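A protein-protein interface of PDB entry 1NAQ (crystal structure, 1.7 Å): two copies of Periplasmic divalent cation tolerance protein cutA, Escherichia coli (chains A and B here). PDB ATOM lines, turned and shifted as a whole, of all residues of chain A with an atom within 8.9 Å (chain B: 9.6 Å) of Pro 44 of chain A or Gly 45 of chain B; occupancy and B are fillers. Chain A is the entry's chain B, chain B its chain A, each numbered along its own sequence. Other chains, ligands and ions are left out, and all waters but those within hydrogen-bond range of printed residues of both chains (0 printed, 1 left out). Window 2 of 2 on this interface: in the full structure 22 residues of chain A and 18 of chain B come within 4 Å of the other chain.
The backbone NH (N) of Leu 42 of chain A lies within hydrogen-bond range of the backbone carbonyl oxygen (O) of Thr 47 of chain B (2.8 Å). The side-chain hydroxyl (OG) of Ser 48 of chain B sits at hydrogen-bond distance from the side-chain hydroxyl (OG1) of Thr 41 of chain A.
N of Glu 61 of chain B lies within hydrogen-bond range of O of Ala 46 of chain B (2.9 Å). The backbone carbonyl oxygen of Ser 48 of chain B sits at hydrogen-bond distance from the backbone NH of Glu 59 of chain B. O of Ile 43 of chain A lies within hydrogen-bond range of N of Gln 63 of chain A, at 2.9 Å.
O of Thr 47 of chain B touches CA of Thr 41 of chain A, at 3.3 Å. O of Gly 45 of chain B touches O of Leu 42 of chain A (3.6 Å). Leu 42 of chain A touches Ala 46 of chain B. O of Gly 45 of chain B touches CA of Ile 43 of chain A (3.97 Å). Pro 44 of chain A touches Gly 45 of chain B.
Pro 44 of chain A touches one residue of chain B. Of chain A, only Leu 42 (3.6 Å), Ile 43 (3.97 Å) and Pro 44 (3.2 Å) come within 4 Å of Gly 45 of chain B. No residue of chain B comes within 4 Å of Gly 45 of chain A. No residue of chain A comes within 4 Å of Pro 44 of chain B. Printed residues of chain A within 4 Å of Ser 48 of chain B: Thr 41 (2.7 Å). Printed residues of chain B within 4 Å of Leu 42 of chain A: Gly 45 (3.6 Å), Ala 46 (3.2 Å) and Thr 47 (2.8 Å). Glu 61 of chain B touches none of the printed residues of chain A. Gln 63 of chain B touches none of the printed residues of chain A. The nearest residue of chain B that does not touch Pro 44 of chain A is Ala 46 of chain B (5.2 Å).
Of the 17 printed residues of chain B, 4 touch a printed residue of chain A. Of the 18 printed residues of chain A, 4 touch a printed residue of chain B. Printed residues of chain A that touch a printed residue of chain B: Thr 41, Leu 42, Ile 43 and Pro 44. Hydrophobic or aromatic side chains of chain A within 4 Å of the printed part of chain B: Leu 42 and Pro 44. Along chain A the printed residues that touch a printed residue of chain B span positions 41 to 44.
Leu 42 of chain A touches Gly 45 of chain B, but with the chains exchanged Gly 45 of chain A does not touch Leu 42 of chain B (12.7 Å). Leu 42 of chain A touches Ala 46 of chain B, but with the chains exchanged Ala 46 of chain A does not touch Leu 42 of chain B (12.9 Å). Leu 42 of chain A touches Thr 47 of chain B, but with the chains exchanged Thr 47 of chain A does not touch Leu 42 of chain B (14.4 Å). Pro 44 of chain A touches Gly 45 of chain B, but with the chains exchanged Gly 45 of chain A does not touch Pro 44 of chain B (8.3 Å). Of the 7 pairs that touch across the chains among the printed residues, none has its exchanged pair printed and touching as well.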
ATOM      1  N   ALA A  18     -21.449  25.870   6.697  1.00  0.00           N
ATOM      2  CA  ALA A  18     -20.184  25.886   5.985  1.00  0.00           C
ATOM      3  C   ALA A  18     -19.502  24.527   6.324  1.00  0.00           C
ATOM      4  O   ALA A  18     -19.779  23.913   7.342  1.00  0.00           O
ATOM      5  CB  ALA A  18     -19.306  27.067   6.439  1.00  0.00           C
ATOM      6  N   PRO A  19     -18.772  23.970   5.360  1.00  0.00           N
ATOM      7  CA  PRO A  19     -18.051  22.696   5.524  1.00  0.00           C
ATOM      8  C   PRO A  19     -16.889  22.619   6.461  1.00  0.00           C
ATOM      9  O   PRO A  19     -16.582  21.490   6.894  1.00  0.00           O
ATOM     10  CB  PRO A  19     -17.461  22.462   4.133  1.00  0.00           C
ATOM     11  CG  PRO A  19     -17.462  23.758   3.505  1.00  0.00           C
ATOM     12  CD  PRO A  19     -18.783  24.395   3.950  1.00  0.00           C
ATOM     13  N   ASP A  20     -16.244  23.739   6.748  1.00  0.00           N
ATOM     14  CA  ASP A  20     -15.107  23.758   7.651  1.00  0.00           C
ATOM     15  C   ASP A  20     -14.884  25.174   8.129  1.00  0.00           C
ATOM     16  O   ASP A  20     -15.360  26.114   7.503  1.00  0.00           O
ATOM     17  CB  ASP A  20     -13.876  23.312   6.885  1.00  0.00           C
ATOM     18  CG  ASP A  20     -13.606  24.199   5.688  1.00  0.00           C
ATOM     19  OD1 ASP A  20     -12.652  24.985   5.737  1.00  0.00           O
ATOM     20  OD2 ASP A  20     -14.310  24.197   4.664  1.00  0.00           O
ATOM     21  N   GLU A  21     -14.154  25.331   9.230  1.00  0.00           N
ATOM     22  CA  GLU A  21     -13.965  26.658   9.802  1.00  0.00           C
ATOM     23  C   GLU A  21     -13.185  27.647   8.926  1.00  0.00           C
ATOM     24  O   GLU A  21     -13.324  28.862   9.097  1.00  0.00           O
ATOM     25  CB  GLU A  21     -13.369  26.609  11.218  1.00  0.00           C
ATOM     26  CG  GLU A  21     -12.228  25.644  11.400  1.00  0.00           C
ATOM     27  CD  GLU A  21     -12.524  24.610  12.473  1.00  0.00           C
ATOM     28  OE1 GLU A  21     -12.969  23.479  12.166  1.00  0.00           O
ATOM     29  OE2 GLU A  21     -12.332  24.942  13.646  1.00  0.00           O
ATOM     30  N   ALA A  22     -12.391  27.139   7.985  1.00  0.00           N
ATOM     31  CA  ALA A  22     -11.642  27.989   7.097  1.00  0.00           C
ATOM     32  C   ALA A  22     -12.513  28.677   6.029  1.00  0.00           C
ATOM     33  O   ALA A  22     -12.350  29.869   5.803  1.00  0.00           O
ATOM     34  CB  ALA A  22     -10.456  27.214   6.452  1.00  0.00           C
ATOM     35  N   ALA A  24     -15.758  28.967   6.336  1.00  0.00           N
ATOM     36  CA  ALA A  24     -16.696  29.722   7.185  1.00  0.00           C
ATOM     37  C   ALA A  24     -16.159  31.085   7.629  1.00  0.00           C
ATOM     38  O   ALA A  24     -16.873  32.065   7.566  1.00  0.00           O
ATOM     39  CB  ALA A  24     -17.096  28.871   8.394  1.00  0.00           C
ATOM     40  N   THR A  41     -21.187  34.799  13.751  1.00  0.00           N
ATOM     41  CA  THR A  41     -20.774  33.844  14.758  1.00  0.00           C
ATOM     42  C   THR A  41     -20.636  32.461  14.177  1.00  0.00           C
ATOM     43  O   THR A  41     -21.518  32.001  13.438  1.00  0.00           O
ATOM     44  CB  THR A  41     -21.820  33.864  15.900  1.00  0.00           C
ATOM     45  OG1 THR A  41     -21.757  35.156  16.516  1.00  0.00           O
ATOM     46  CG2 THR A  41     -21.401  32.899  16.985  1.00  0.00           C
ATOM     47  N   LEU A  42     -19.530  31.804  14.501  1.00  0.00           N
ATOM     48  CA  LEU A  42     -19.220  30.457  13.956  1.00  0.00           C
ATOM     49  C   LEU A  42     -19.071  29.435  15.091  1.00  0.00           C
ATOM     50  O   LEU A  42     -18.353  29.698  16.064  1.00  0.00           O
ATOM     51  CB  LEU A  42     -17.873  30.515  13.228  1.00  0.00           C
ATOM     52  CG  LEU A  42     -17.698  31.553  12.099  1.00  0.00           C
ATOM     53  CD1 LEU A  42     -16.290  31.461  11.470  1.00  0.00           C
ATOM     54  CD2 LEU A  42     -18.822  31.695  11.080  1.00  0.00           C
ATOM     55  N   ILE A  43     -19.727  28.277  14.949  1.00  0.00           N
ATOM     56  CA  ILE A  43     -19.603  27.177  15.875  1.00  0.00           C
ATOM     57  C   ILE A  43     -19.209  25.962  15.078  1.00  0.00           C
ATOM     58  O   ILE A  43     -20.062  25.338  14.468  1.00  0.00           O
ATOM     59  CB  ILE A  43     -20.967  26.957  16.618  1.00  0.00           C
ATOM     60  CG1 ILE A  43     -21.485  28.285  17.210  1.00  0.00           C
ATOM     61  CG2 ILE A  43     -20.864  25.914  17.778  1.00  0.00           C
ATOM     62  CD1 ILE A  43     -22.894  28.196  17.909  1.00  0.00           C
ATOM     63  N   PRO A  44     -17.917  25.648  15.046  1.00  0.00           N
ATOM     64  CA  PRO A  44     -17.443  24.430  14.360  1.00  0.00           C
ATOM     65  C   PRO A  44     -17.673  23.212  15.275  1.00  0.00           C
ATOM     66  O   PRO A  44     -18.078  23.334  16.459  1.00  0.00           O
ATOM     67  CB  PRO A  44     -15.948  24.694  14.213  1.00  0.00           C
ATOM     68  CG  PRO A  44     -15.627  25.489  15.455  1.00  0.00           C
ATOM     69  CD  PRO A  44     -16.830  26.349  15.756  1.00  0.00           C
ATOM     70  N   GLY A  45     -17.426  22.024  14.740  1.00  0.00           N
ATOM     71  CA  GLY A  45     -17.493  20.812  15.534  1.00  0.00           C
ATOM     72  C   GLY A  45     -18.897  20.205  15.541  1.00  0.00           C
ATOM     73  O   GLY A  45     -19.124  19.223  16.205  1.00  0.00           O
ATOM     74  N   ALA A  46     -19.834  20.824  14.827  1.00  0.00           N
ATOM     75  CA  ALA A  46     -21.171  20.279  14.672  1.00  0.00           C
ATOM     76  C   ALA A  46     -21.195  19.046  13.775  1.00  0.00           C
ATOM     77  O   ALA A  46     -20.324  18.865  12.944  1.00  0.00           O
ATOM     78  CB  ALA A  46     -22.080  21.373  14.150  1.00  0.00           C
ATOM     79  N   THR A  47     -22.152  18.171  14.013  1.00  0.00           N
ATOM     80  CA  THR A  47     -22.407  17.040  13.135  1.00  0.00           C
ATOM     81  C   THR A  47     -23.729  17.269  12.438  1.00  0.00           C
ATOM     82  O   THR A  47     -24.740  17.566  13.083  1.00  0.00           O
ATOM     83  CB  THR A  47     -22.477  15.705  13.924  1.00  0.00           C
ATOM     84  OG1 THR A  47     -21.191  15.368  14.494  1.00  0.00           O
ATOM     85  CG2 THR A  47     -22.767  14.546  12.986  1.00  0.00           C
ATOM     86  N   TYR A  60     -18.967  16.374   9.489  1.00  0.00           N
ATOM     87  CA  TYR A  60     -18.768  17.528  10.398  1.00  0.00           C
ATOM     88  C   TYR A  60     -19.122  18.847   9.692  1.00  0.00           C
ATOM     89  O   TYR A  60     -18.985  18.977   8.488  1.00  0.00           O
ATOM     90  CB  TYR A  60     -17.393  17.579  11.042  1.00  0.00           C
ATOM     91  CG  TYR A  60     -17.161  16.455  11.980  1.00  0.00           C
ATOM     92  CD1 TYR A  60     -17.630  16.511  13.291  1.00  0.00           C
ATOM     93  CD2 TYR A  60     -16.573  15.286  11.537  1.00  0.00           C
ATOM     94  CE1 TYR A  60     -17.468  15.440  14.142  1.00  0.00           C
ATOM     95  CE2 TYR A  60     -16.400  14.214  12.367  1.00  0.00           C
ATOM     96  CZ  TYR A  60     -16.838  14.294  13.674  1.00  0.00           C
ATOM     97  OH  TYR A  60     -16.650  13.225  14.489  1.00  0.00           O
ATOM     98  N   GLU A  61     -19.617  19.815  10.455  1.00  0.00           N
ATOM     99  CA  GLU A  61     -20.042  21.093   9.864  1.00  0.00           C
ATOM    100  C   GLU A  61     -19.797  22.235  10.869  1.00  0.00           C
ATOM    101  O   GLU A  61     -19.597  21.988  12.042  1.00  0.00           O
ATOM    102  CB  GLU A  61     -21.515  21.041   9.517  1.00  0.00           C
ATOM    103  CG  GLU A  61     -21.988  19.761   8.830  1.00  0.00           C
ATOM    104  CD  GLU A  61     -21.827  19.812   7.294  1.00  0.00           C
ATOM    105  OE1 GLU A  61     -21.224  20.765   6.764  1.00  0.00           O
ATOM    106  OE2 GLU A  61     -22.281  18.867   6.606  1.00  0.00           O
ATOM    107  N   VAL A  62     -19.832  23.449  10.360  1.00  0.00           N
ATOM    108  CA  VAL A  62     -19.755  24.655  11.138  1.00  0.00           C
ATOM    109  C   VAL A  62     -21.072  25.384  10.972  1.00  0.00           C
ATOM    110  O   VAL A  62     -21.479  25.743   9.864  1.00  0.00           O
ATOM    111  CB  VAL A  62     -18.602  25.591  10.677  1.00  0.00           C
ATOM    112  CG1 VAL A  62     -18.671  26.966  11.375  1.00  0.00           C
ATOM    113  CG2 VAL A  62     -17.226  24.902  10.886  1.00  0.00           C
ATOM    114  N   GLN A  63     -21.733  25.608  12.114  1.00  0.00           N
ATOM    115  CA  GLN A  63     -22.974  26.347  12.183  1.00  0.00           C
ATOM    116  C   GLN A  63     -22.677  27.862  12.163  1.00  0.00           C
ATOM    117  O   GLN A  63     -21.858  28.340  12.973  1.00  0.00           O
ATOM    118  CB  GLN A  63     -23.775  25.961  13.460  1.00  0.00           C
ATOM    119  CG  GLN A  63     -25.144  26.667  13.610  1.00  0.00           C
ATOM    120  CD  GLN A  63     -26.056  26.484  12.396  1.00  0.00           C
ATOM    121  OE1 GLN A  63     -26.283  27.437  11.605  1.00  0.00           O
ATOM    122  NE2 GLN A  63     -26.615  25.295  12.247  1.00  0.00           N
ATOM    123  N   MET A  64     -23.308  28.618  11.253  1.00  0.00           N
ATOM    124  CA  MET A  64     -23.054  30.053  11.188  1.00  0.00           C
ATOM    125  C   MET A  64     -24.293  30.703  11.737  1.00  0.00           C
ATOM    126  O   MET A  64     -25.404  30.202  11.462  1.00  0.00           O
ATOM    127  CB  MET A  64     -22.779  30.579   9.787  1.00  0.00           C
ATOM    128  CG  MET A  64     -21.572  29.876   9.106  1.00  0.00           C
ATOM    129  SD  MET A  64     -21.103  30.458   7.500  1.00  0.00           S
ATOM    130  CE  MET A  64     -20.469  31.978   7.959  1.00  0.00           C
ATOM    131  N   ALA B  18     -21.486  35.611  26.167  1.00  0.00           N
ATOM    132  CA  ALA B  18     -20.545  35.691  27.320  1.00  0.00           C
ATOM    133  C   ALA B  18     -19.111  35.317  26.853  1.00  0.00           C
ATOM    134  O   ALA B  18     -18.963  34.611  25.850  1.00  0.00           O
ATOM    135  CB  ALA B  18     -20.987  34.799  28.482  1.00  0.00           C
ATOM    136  N   PRO B  19     -18.064  35.833  27.483  1.00  0.00           N
ATOM    137  CA  PRO B  19     -16.709  35.578  26.962  1.00  0.00           C
ATOM    138  C   PRO B  19     -16.146  34.174  27.260  1.00  0.00           C
ATOM    139  O   PRO B  19     -15.272  33.662  26.497  1.00  0.00           O
ATOM    140  CB  PRO B  19     -15.829  36.634  27.639  1.00  0.00           C
ATOM    141  CG  PRO B  19     -16.697  37.336  28.685  1.00  0.00           C
ATOM    142  CD  PRO B  19     -18.095  36.711  28.680  1.00  0.00           C
ATOM    143  N   ASP B  20     -16.609  33.585  28.352  1.00  0.00           N
ATOM    144  CA  ASP B  20     -16.030  32.355  28.860  1.00  0.00           C
ATOM    145  C   ASP B  20     -16.986  31.577  29.801  1.00  0.00           C
ATOM    146  O   ASP B  20     -18.036  32.055  30.145  1.00  0.00           O
ATOM    147  CB  ASP B  20     -14.653  32.655  29.445  1.00  0.00           C
ATOM    148  CG  ASP B  20     -14.718  33.435  30.768  1.00  0.00           C
ATOM    149  OD1 ASP B  20     -15.712  33.370  31.494  1.00  0.00           O
ATOM    150  OD2 ASP B  20     -13.784  34.150  31.121  1.00  0.00           O
ATOM    151  N   GLU B  21     -16.625  30.356  30.170  1.00  0.00           N
ATOM    152  CA  GLU B  21     -17.544  29.492  30.871  1.00  0.00           C
ATOM    153  C   GLU B  21     -17.807  30.021  32.256  1.00  0.00           C
ATOM    154  O   GLU B  21     -18.964  30.004  32.708  1.00  0.00           O
ATOM    155  CB  GLU B  21     -16.980  28.068  30.878  1.00  0.00           C
ATOM    156  CG  GLU B  21     -17.136  27.431  29.528  1.00  0.00           C
ATOM    157  CD  GLU B  21     -18.410  26.626  29.322  1.00  0.00           C
ATOM    158  OE1 GLU B  21     -19.356  26.698  30.154  1.00  0.00           O
ATOM    159  OE2 GLU B  21     -18.478  25.905  28.279  1.00  0.00           O
ATOM    160  N   LEU B  42     -25.487  26.710  27.812  1.00  0.00           N
ATOM    161  CA  LEU B  42     -24.248  27.384  27.392  1.00  0.00           C
ATOM    162  C   LEU B  42     -23.591  26.595  26.273  1.00  0.00           C
ATOM    163  O   LEU B  42     -23.312  25.394  26.431  1.00  0.00           O
ATOM    164  CB  LEU B  42     -23.277  27.576  28.587  1.00  0.00           C
ATOM    165  CG  LEU B  42     -23.900  28.147  29.859  1.00  0.00           C
ATOM    166  CD1 LEU B  42     -22.844  28.314  30.903  1.00  0.00           C
ATOM    167  CD2 LEU B  42     -24.681  29.401  29.585  1.00  0.00           C
ATOM    168  N   ILE B  43     -23.317  27.224  25.139  1.00  0.00           N
ATOM    169  CA  ILE B  43     -22.594  26.541  24.026  1.00  0.00           C
ATOM    170  C   ILE B  43     -21.181  27.122  23.822  1.00  0.00           C
ATOM    171  O   ILE B  43     -21.045  28.237  23.354  1.00  0.00           O
ATOM    172  CB  ILE B  43     -23.428  26.582  22.765  1.00  0.00           C
ATOM    173  CG1 ILE B  43     -24.816  26.039  23.055  1.00  0.00           C
ATOM    174  CG2 ILE B  43     -22.832  25.715  21.656  1.00  0.00           C
ATOM    175  CD1 ILE B  43     -25.735  26.045  21.886  1.00  0.00           C
ATOM    176  N   PRO B  44     -20.148  26.407  24.238  1.00  0.00           N
ATOM    177  CA  PRO B  44     -18.752  26.838  24.038  1.00  0.00           C
ATOM    178  C   PRO B  44     -18.293  26.609  22.602  1.00  0.00           C
ATOM    179  O   PRO B  44     -19.007  25.967  21.853  1.00  0.00           O
ATOM    180  CB  PRO B  44     -17.995  25.905  24.981  1.00  0.00           C
ATOM    181  CG  PRO B  44     -18.731  24.687  24.817  1.00  0.00           C
ATOM    182  CD  PRO B  44     -20.193  25.148  25.026  1.00  0.00           C
ATOM    183  N   GLY B  45     -17.124  27.139  22.208  1.00  0.00           N
ATOM    184  CA  GLY B  45     -16.660  26.895  20.848  1.00  0.00           C
ATOM    185  C   GLY B  45     -17.029  27.959  19.791  1.00  0.00           C
ATOM    186  O   GLY B  45     -16.792  27.740  18.619  1.00  0.00           O
ATOM    187  N   ALA B  46     -17.698  29.036  20.176  1.00  0.00           N
ATOM    188  CA  ALA B  46     -18.159  30.049  19.242  1.00  0.00           C
ATOM    189  C   ALA B  46     -17.037  31.023  18.996  1.00  0.00           C
ATOM    190  O   ALA B  46     -16.267  31.352  19.930  1.00  0.00           O
ATOM    191  CB  ALA B  46     -19.412  30.820  19.802  1.00  0.00           C
ATOM    192  N   THR B  47     -16.938  31.514  17.752  1.00  0.00           N
ATOM    193  CA  THR B  47     -16.062  32.641  17.443  1.00  0.00           C
ATOM    194  C   THR B  47     -16.916  33.680  16.816  1.00  0.00           C
ATOM    195  O   THR B  47     -17.666  33.387  15.875  1.00  0.00           O
ATOM    196  CB  THR B  47     -14.925  32.265  16.440  1.00  0.00           C
ATOM    197  OG1 THR B  47     -13.989  31.338  17.024  1.00  0.00           O
ATOM    198  CG2 THR B  47     -14.014  33.478  16.073  1.00  0.00           C
ATOM    199  N   SER B  48     -16.762  34.914  17.275  1.00  0.00           N
ATOM    200  CA  SER B  48     -17.424  36.003  16.552  1.00  0.00           C
ATOM    201  C   SER B  48     -16.514  36.960  15.849  1.00  0.00           C
ATOM    202  O   SER B  48     -15.426  37.276  16.348  1.00  0.00           O
ATOM    203  CB  SER B  48     -18.326  36.729  17.458  1.00  0.00           C
ATOM    204  OG  SER B  48     -19.463  35.913  17.657  1.00  0.00           O
ATOM    205  N   GLN B  58     -11.965  39.374  15.910  1.00  0.00           N
ATOM    206  CA  GLN B  58     -12.307  37.972  15.946  1.00  0.00           C
ATOM    207  C   GLN B  58     -12.184  37.654  17.414  1.00  0.00           C
ATOM    208  O   GLN B  58     -11.182  38.034  18.063  1.00  0.00           O
ATOM    209  CB  GLN B  58     -11.377  37.105  15.095  1.00  0.00           C
ATOM    210  CG  GLN B  58     -12.039  35.747  14.671  1.00  0.00           C
ATOM    211  CD  GLN B  58     -11.234  34.865  13.701  1.00  0.00           C
ATOM    212  OE1 GLN B  58     -11.063  35.188  12.516  1.00  0.00           O
ATOM    213  NE2 GLN B  58     -10.788  33.706  14.202  1.00  0.00           N
ATOM    214  N   GLU B  59     -13.244  37.096  18.003  1.00  0.00           N
ATOM    215  CA  GLU B  59     -13.149  36.841  19.412  1.00  0.00           C
ATOM    216  C   GLU B  59     -13.849  35.544  19.814  1.00  0.00           C
ATOM    217  O   GLU B  59     -14.916  35.222  19.292  1.00  0.00           O
ATOM    218  CB  GLU B  59     -13.715  38.016  20.198  1.00  0.00           C
ATOM    219  CG  GLU B  59     -13.060  39.353  19.850  1.00  0.00           C
ATOM    220  CD  GLU B  59     -11.939  39.761  20.802  1.00  0.00           C
ATOM    221  OE1 GLU B  59     -12.151  40.683  21.643  1.00  0.00           O
ATOM    222  OE2 GLU B  59     -10.831  39.189  20.702  1.00  0.00           O
ATOM    223  N   TYR B  60     -13.272  34.843  20.781  1.00  0.00           N
ATOM    224  CA  TYR B  60     -13.921  33.676  21.322  1.00  0.00           C
ATOM    225  C   TYR B  60     -15.049  33.983  22.302  1.00  0.00           C
ATOM    226  O   TYR B  60     -14.921  34.892  23.141  1.00  0.00           O
ATOM    227  CB  TYR B  60     -12.860  32.826  22.042  1.00  0.00           C
ATOM    228  CG  TYR B  60     -11.817  32.192  21.134  1.00  0.00           C
ATOM    229  CD1 TYR B  60     -10.457  32.417  21.351  1.00  0.00           C
ATOM    230  CD2 TYR B  60     -12.191  31.351  20.068  1.00  0.00           C
ATOM    231  CE1 TYR B  60      -9.470  31.815  20.537  1.00  0.00           C
ATOM    232  CE2 TYR B  60     -11.221  30.729  19.268  1.00  0.00           C
ATOM    233  CZ  TYR B  60      -9.861  30.987  19.514  1.00  0.00           C
ATOM    234  OH  TYR B  60      -8.909  30.406  18.752  1.00  0.00           O
ATOM    235  N   GLU B  61     -16.126  33.204  22.196  1.00  0.00           N
ATOM    236  CA  GLU B  61     -17.374  33.460  22.920  1.00  0.00           C
ATOM    237  C   GLU B  61     -18.039  32.164  23.402  1.00  0.00           C
ATOM    238  O   GLU B  61     -17.741  31.028  22.934  1.00  0.00           O
ATOM    239  CB  GLU B  61     -18.392  34.267  22.108  1.00  0.00           C
ATOM    240  CG  GLU B  61     -17.886  35.350  21.133  1.00  0.00           C
ATOM    241  CD  GLU B  61     -17.641  36.678  21.837  1.00  0.00           C
ATOM    242  OE1 GLU B  61     -17.814  36.737  23.092  1.00  0.00           O
ATOM    243  OE2 GLU B  61     -17.296  37.670  21.130  1.00  0.00           O
ATOM    244  N   VAL B  62     -18.911  32.341  24.388  1.00  0.00           N
ATOM    245  CA  VAL B  62     -19.774  31.243  24.837  1.00  0.00           C
ATOM    246  C   VAL B  62     -21.183  31.781  24.483  1.00  0.00           C
ATOM    247  O   VAL B  62     -21.548  32.869  24.924  1.00  0.00           O
ATOM    248  CB  VAL B  62     -19.674  30.973  26.343  1.00  0.00           C
ATOM    249  CG1 VAL B  62     -20.822  30.130  26.838  1.00  0.00           C
ATOM    250  CG2 VAL B  62     -18.311  30.344  26.722  1.00  0.00           C
ATOM    251  N   GLN B  63     -21.936  31.041  23.660  1.00  0.00           N
ATOM    252  CA  GLN B  63     -23.266  31.391  23.297  1.00  0.00           C
ATOM    253  C   GLN B  63     -24.304  30.928  24.352  1.00  0.00           C
ATOM    254  O   GLN B  63     -24.367  29.722  24.656  1.00  0.00           O
ATOM    255  CB  GLN B  63     -23.602  30.824  21.900  1.00  0.00           C
ATOM    256  CG  GLN B  63     -25.055  31.116  21.460  1.00  0.00           C
ATOM    257  CD  GLN B  63     -25.306  32.584  21.117  1.00  0.00           C
ATOM    258  OE1 GLN B  63     -24.788  33.074  20.112  1.00  0.00           O
ATOM    259  NE2 GLN B  63     -26.088  33.283  21.925  1.00  0.00           N
